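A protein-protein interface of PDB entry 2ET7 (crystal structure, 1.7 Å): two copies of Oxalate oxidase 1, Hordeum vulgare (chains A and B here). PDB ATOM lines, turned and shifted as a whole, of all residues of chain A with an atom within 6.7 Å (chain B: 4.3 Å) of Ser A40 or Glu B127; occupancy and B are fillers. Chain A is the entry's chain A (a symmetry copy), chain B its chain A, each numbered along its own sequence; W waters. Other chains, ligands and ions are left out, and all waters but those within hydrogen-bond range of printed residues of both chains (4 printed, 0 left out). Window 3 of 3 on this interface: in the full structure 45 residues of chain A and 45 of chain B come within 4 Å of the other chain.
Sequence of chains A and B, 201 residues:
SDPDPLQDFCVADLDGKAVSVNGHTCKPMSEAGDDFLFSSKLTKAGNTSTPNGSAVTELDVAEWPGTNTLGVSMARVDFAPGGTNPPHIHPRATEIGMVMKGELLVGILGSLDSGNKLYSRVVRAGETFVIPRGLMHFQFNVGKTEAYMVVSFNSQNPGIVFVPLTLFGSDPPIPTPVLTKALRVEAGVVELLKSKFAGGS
N of Thr B128 is in hydrogen-bond range of O of Ser A39 (2.8 Å).
O of Val B99 sits at hydrogen-bond distance from N of Gly B126 (2.8 Å). The backbone NH of Val B99 is in hydrogen-bond range of the backbone carbonyl oxygen of Glu B127 (3.1 Å). The backbone NH of Arg B124 lies within hydrogen-bond range of the side-chain carboxylate of Glu B127, at 2.8 Å. The side-chain hydroxyl of Ser A39 lies within hydrogen-bond range of the backbone NH of Lys A41, 3.2 Å away. The side-chain hydroxyl (OG1) of Thr A43 lies within hydrogen-bond range of the backbone carbonyl oxygen (O) of Ser A40 (2.9 Å).
Among the printed residues, merely in contact across the chains: Phe A38 with Val B123 (3.9 Å), Phe A38 with Thr B128 (3.4 Å), Ser A39 with Glu B127 (3.5 Å), Ser A40 with Glu B127 (3.7 Å), Leu A42 with Met B98 (3.7 Å), Leu A42 with Gly B126 (3.8 Å), Thr A43 with Ala B125 (3.7 Å), Thr A43 with Gly B126 (3.7 Å), Thr A43 with Glu B127 (3.7 Å) and Leu A59 with Thr B128 (3.5 Å).
Glu B127 touches just these residues of chain A: Ser A39 (3.5 Å), Ser A40 (3.7 Å) and Thr A43 (3.7 Å). Printed residues of chain B within 4 Å of Leu A59: Thr B128. Of the printed residues of chain A, Gly B126 touches Leu A42 and Thr A43. Lys A41 touches none of the printed residues of chain B. Lys A44 touches none of the printed residues of chain B. The nearest residue of chain A that does not touch Glu B127 is Leu A42 (5.7 Å). The nearest printed residue of chain A that does not touch Met B98 is Thr A43 (5.8 Å).
Hydrophobic or aromatic side chains of chain A that line the printed part of chain B: Phe A38, Leu A42 and Leu A59. Along chain A the printed residues that touch a printed residue of chain B span positions 38 to 59. Of the 10 printed residues of chain B, 6 touch a printed residue of chain A. Hydrophobic or aromatic side chains of chain B within 4 Å of the printed part of chain A: Met B98 and Val B123. Among the printed residues, no Asp or Glu carboxylate lies within 4 Å of a Lys or Arg side-chain nitrogen of the other chain.
No position is printed for both chains.
Water W2 bridges O of Leu A42 (2.7 Å) and SD of Met B98 (3.5 Å). Water W1 lies within hydrogen-bond range of the backbone carbonyl oxygen (O) of Gly B126 (2.8 Å), the backbone NH (N) of Leu A42 (2.9 Å), the backbone carbonyl oxygen (O) of Ser A39 (3.3 Å), the backbone NH (N) of Lys A41 (3.3 Å) and the side-chain hydroxyl (OG1) of Thr B128 (3.4 Å). Water W4 lies within hydrogen-bond range of O of Thr B128 (2.9 Å) and O of Ser A39 (3.2 Å). Water W3 bridges the backbone carbonyl oxygen (O) of Ala B125 and the backbone carbonyl oxygen (O) of Thr A43.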
ATOM      1  N   PHE A  38       9.800 -20.369  16.097  1.00  0.00           N
ATOM      2  CA  PHE A  38       8.549 -21.164  16.092  1.00  0.00           C
ATOM      3  C   PHE A  38       7.300 -20.311  15.917  1.00  0.00           C
ATOM      4  O   PHE A  38       7.271 -19.158  16.351  1.00  0.00           O
ATOM      5  CB  PHE A  38       8.445 -21.958  17.389  1.00  0.00           C
ATOM      6  CG  PHE A  38       9.634 -22.830  17.641  1.00  0.00           C
ATOM      7  CD1 PHE A  38      10.675 -22.391  18.460  1.00  0.00           C
ATOM      8  CD2 PHE A  38       9.736 -24.084  17.026  1.00  0.00           C
ATOM      9  CE1 PHE A  38      11.807 -23.180  18.681  1.00  0.00           C
ATOM     10  CE2 PHE A  38      10.853 -24.896  17.236  1.00  0.00           C
ATOM     11  CZ  PHE A  38      11.900 -24.442  18.065  1.00  0.00           C
ATOM     12  N   SER A  39       6.262 -20.886  15.308  1.00  0.00           N
ATOM     13  CA  SER A  39       4.972 -20.207  15.234  1.00  0.00           C
ATOM     14  C   SER A  39       3.830 -21.211  15.291  1.00  0.00           C
ATOM     15  O   SER A  39       3.995 -22.391  14.925  1.00  0.00           O
ATOM     16  CB  SER A  39       4.865 -19.375  13.957  1.00  0.00           C
ATOM     17  OG  SER A  39       3.640 -18.649  13.877  1.00  0.00           O
ATOM     18  N   SER A  40       2.676 -20.716  15.730  1.00  0.00           N
ATOM     19  CA  SER A  40       1.456 -21.514  15.719  1.00  0.00           C
ATOM     20  C   SER A  40       0.345 -20.813  14.928  1.00  0.00           C
ATOM     21  O   SER A  40      -0.816 -21.217  14.987  1.00  0.00           O
ATOM     22  CB  SER A  40       1.020 -21.854  17.151  1.00  0.00           C
ATOM     23  OG  SER A  40       0.677 -20.666  17.847  1.00  0.00           O
ATOM     24  N   LYS A  41       0.712 -19.800  14.148  1.00  0.00           N
ATOM     25  CA  LYS A  41      -0.291 -18.989  13.434  1.00  0.00           C
ATOM     26  C   LYS A  41      -1.070 -19.722  12.342  1.00  0.00           C
ATOM     27  O   LYS A  41      -2.133 -19.244  11.925  1.00  0.00           O
ATOM     28  CB  LYS A  41       0.325 -17.687  12.904  1.00  0.00           C
ATOM     29  CG  LYS A  41       0.478 -16.646  14.003  1.00  0.00           C
ATOM     30  CD  LYS A  41       0.997 -15.309  13.474  1.00  0.00           C
ATOM     31  CE  LYS A  41       1.160 -14.322  14.618  1.00  0.00           C
ATOM     32  NZ  LYS A  41       1.800 -13.054  14.183  1.00  0.00           N
ATOM     33  N   LEU A  42      -0.562 -20.864  11.876  1.00  0.00           N
ATOM     34  CA  LEU A  42      -1.250 -21.614  10.813  1.00  0.00           C
ATOM     35  C   LEU A  42      -2.067 -22.807  11.316  1.00  0.00           C
ATOM     36  O   LEU A  42      -2.499 -23.646  10.522  1.00  0.00           O
ATOM     37  CB  LEU A  42      -0.250 -22.066   9.738  1.00  0.00           C
ATOM     38  CG  LEU A  42       0.554 -20.934   9.089  1.00  0.00           C
ATOM     39  CD1 LEU A  42       1.416 -21.500   7.967  1.00  0.00           C
ATOM     40  CD2 LEU A  42      -0.340 -19.807   8.546  1.00  0.00           C
ATOM     41  N   THR A  43      -2.277 -22.891  12.630  1.00  0.00           N
ATOM     42  CA  THR A  43      -2.999 -24.039  13.198  1.00  0.00           C
ATOM     43  C   THR A  43      -4.486 -24.045  12.855  1.00  0.00           C
ATOM     44  O   THR A  43      -5.116 -25.103  12.856  1.00  0.00           O
ATOM     45  CB  THR A  43      -2.857 -24.146  14.739  1.00  0.00           C
ATOM     46  OG1 THR A  43      -3.187 -22.886  15.335  1.00  0.00           O
ATOM     47  CG2 THR A  43      -1.449 -24.546  15.139  1.00  0.00           C
ATOM     48  N   LYS A  44      -5.045 -22.875  12.573  1.00  0.00           N
ATOM     49  CA  LYS A  44      -6.484 -22.757  12.358  1.00  0.00           C
ATOM     50  C   LYS A  44      -6.810 -22.291  10.949  1.00  0.00           C
ATOM     51  O   LYS A  44      -6.083 -21.482  10.368  1.00  0.00           O
ATOM     52  CB  LYS A  44      -7.112 -21.794  13.366  1.00  0.00           C
ATOM     53  CG  LYS A  44      -6.959 -22.192  14.837  1.00  0.00           C
ATOM     54  CD  LYS A  44      -7.518 -21.096  15.731  1.00  0.00           C
ATOM     55  CE  LYS A  44      -7.322 -21.416  17.216  1.00  0.00           C
ATOM     56  NZ  LYS A  44      -7.736 -20.255  18.082  1.00  0.00           N
ATOM     57  N   LEU A  59       2.137 -16.182   6.728  1.00  0.00           N
ATOM     58  CA  LEU A  59       3.215 -16.394   7.678  1.00  0.00           C
ATOM     59  C   LEU A  59       4.520 -15.895   7.057  1.00  0.00           C
ATOM     60  O   LEU A  59       5.495 -16.624   6.912  1.00  0.00           O
ATOM     61  CB  LEU A  59       3.298 -17.855   8.134  1.00  0.00           C
ATOM     62  CG  LEU A  59       3.905 -18.087   9.518  1.00  0.00           C
ATOM     63  CD1 LEU A  59       3.200 -17.311  10.624  1.00  0.00           C
ATOM     64  CD2 LEU A  59       3.944 -19.583   9.861  1.00  0.00           C
ATOM     65  N   GLY B  97       9.223 -25.501   8.097  1.00  0.00           N
ATOM     66  CA  GLY B  97       8.407 -26.707   8.079  1.00  0.00           C
ATOM     67  C   GLY B  97       7.267 -26.699   9.058  1.00  0.00           C
ATOM     68  O   GLY B  97       7.160 -25.806   9.885  1.00  0.00           O
ATOM     69  N   MET B  98       6.413 -27.704   8.934  1.00  0.00           N
ATOM     70  CA  MET B  98       5.214 -27.785   9.748  1.00  0.00           C
ATOM     71  C   MET B  98       5.042 -29.225  10.190  1.00  0.00           C
ATOM     72  O   MET B  98       5.204 -30.143   9.376  1.00  0.00           O
ATOM     73  CB  MET B  98       4.006 -27.353   8.914  1.00  0.00           C
ATOM     74  CG  MET B  98       2.695 -27.344   9.670  1.00  0.00           C
ATOM     75  SD  MET B  98       1.313 -27.022   8.550  1.00  0.00           S
ATOM     76  CE  MET B  98       1.237 -25.253   8.632  1.00  0.00           C
ATOM     77  N   VAL B  99       4.704 -29.419  11.461  1.00  0.00           N
ATOM     78  CA  VAL B  99       4.307 -30.744  11.940  1.00  0.00           C
ATOM     79  C   VAL B  99       2.878 -30.997  11.451  1.00  0.00           C
ATOM     80  O   VAL B  99       2.024 -30.111  11.518  1.00  0.00           O
ATOM     81  CB  VAL B  99       4.456 -30.858  13.501  1.00  0.00           C
ATOM     82  CG1 VAL B  99       3.750 -32.122  14.029  1.00  0.00           C
ATOM     83  CG2 VAL B  99       5.945 -30.860  13.883  1.00  0.00           C
ATOM     84  N   VAL B 122       8.183 -28.378  21.924  1.00  0.00           N
ATOM     85  CA  VAL B 122       7.338 -29.432  21.395  1.00  0.00           C
ATOM     86  C   VAL B 122       6.401 -28.820  20.358  1.00  0.00           C
ATOM     87  O   VAL B 122       5.613 -27.907  20.646  1.00  0.00           O
ATOM     88  CB  VAL B 122       6.561 -30.150  22.515  1.00  0.00           C
ATOM     89  CG1 VAL B 122       5.600 -31.164  21.918  1.00  0.00           C
ATOM     90  CG2 VAL B 122       7.553 -30.834  23.444  1.00  0.00           C
ATOM     91  N   VAL B 123       6.522 -29.305  19.131  1.00  0.00           N
ATOM     92  CA  VAL B 123       5.781 -28.755  18.010  1.00  0.00           C
ATOM     93  C   VAL B 123       4.689 -29.735  17.617  1.00  0.00           C
ATOM     94  O   VAL B 123       4.969 -30.916  17.358  1.00  0.00           O
ATOM     95  CB  VAL B 123       6.728 -28.460  16.812  1.00  0.00           C
ATOM     96  CG1 VAL B 123       5.943 -27.807  15.658  1.00  0.00           C
ATOM     97  CG2 VAL B 123       7.889 -27.557  17.256  1.00  0.00           C
ATOM     98  N   ARG B 124       3.451 -29.238  17.589  1.00  0.00           N
ATOM     99  CA  ARG B 124       2.280 -30.070  17.329  1.00  0.00           C
ATOM    100  C   ARG B 124       1.623 -29.749  15.980  1.00  0.00           C
ATOM    101  O   ARG B 124       2.068 -28.858  15.270  1.00  0.00           O
ATOM    102  CB  ARG B 124       1.270 -29.922  18.468  1.00  0.00           C
ATOM    103  CG  ARG B 124       1.747 -30.580  19.757  1.00  0.00           C
ATOM    104  CD  ARG B 124       0.655 -30.556  20.815  1.00  0.00           C
ATOM    105  NE  ARG B 124       1.019 -31.362  21.980  1.00  0.00           N
ATOM    106  CZ  ARG B 124       1.760 -30.921  22.992  1.00  0.00           C
ATOM    107  NH1 ARG B 124       2.222 -29.672  22.997  1.00  0.00           N
ATOM    108  NH2 ARG B 124       2.037 -31.728  24.005  1.00  0.00           N
ATOM    109  N   ALA B 125       0.564 -30.483  15.627  1.00  0.00           N
ATOM    110  CA  ALA B 125      -0.063 -30.330  14.300  1.00  0.00           C
ATOM    111  C   ALA B 125      -0.402 -28.886  13.944  1.00  0.00           C
ATOM    112  O   ALA B 125      -1.051 -28.158  14.715  1.00  0.00           O
ATOM    113  CB  ALA B 125      -1.303 -31.219  14.169  1.00  0.00           C
ATOM    114  N   GLY B 126       0.076 -28.468  12.775  1.00  0.00           N
ATOM    115  CA  GLY B 126      -0.173 -27.122  12.279  1.00  0.00           C
ATOM    116  C   GLY B 126       0.865 -26.089  12.695  1.00  0.00           C
ATOM    117  O   GLY B 126       0.908 -24.988  12.138  1.00  0.00           O
ATOM    118  N   GLU B 127       1.699 -26.437  13.673  1.00  0.00           N
ATOM    119  CA  GLU B 127       2.734 -25.521  14.167  1.00  0.00           C
ATOM    120  C   GLU B 127       4.001 -25.609  13.326  1.00  0.00           C
ATOM    121  O   GLU B 127       4.300 -26.658  12.745  1.00  0.00           O
ATOM    122  CB  GLU B 127       3.043 -25.777  15.648  1.00  0.00           C
ATOM    123  CG  GLU B 127       1.807 -25.558  16.514  1.00  0.00           C
ATOM    124  CD  GLU B 127       2.047 -25.794  18.003  1.00  0.00           C
ATOM    125  OE1 GLU B 127       2.941 -26.575  18.383  1.00  0.00           O
ATOM    126  OE2 GLU B 127       1.324 -25.154  18.807  1.00  0.00           O
ATOM    127  N   THR B 128       4.755 -24.512  13.292  1.00  0.00           N
ATOM    128  CA  THR B 128       5.871 -24.396  12.337  1.00  0.00           C
ATOM    129  C   THR B 128       7.182 -24.027  13.005  1.00  0.00           C
ATOM    130  O   THR B 128       7.206 -23.534  14.125  1.00  0.00           O
ATOM    131  CB  THR B 128       5.565 -23.358  11.239  1.00  0.00           C
ATOM    132  OG1 THR B 128       5.211 -22.110  11.841  1.00  0.00           O
ATOM    133  CG2 THR B 128       4.390 -23.827  10.353  1.00  0.00           C
HETATM  134  O   HOH W   1       1.871 -22.345  12.459  1.00  0.00           O
HETATM  135  O   HOH W   2      -1.935 -25.768   8.882  1.00  0.00           O
HETATM  136  O   HOH W   3      -3.773 -27.794  13.522  1.00  0.00           O
HETATM  137  O   HOH W   4       5.961 -24.153  16.690  1.00  0.00           O
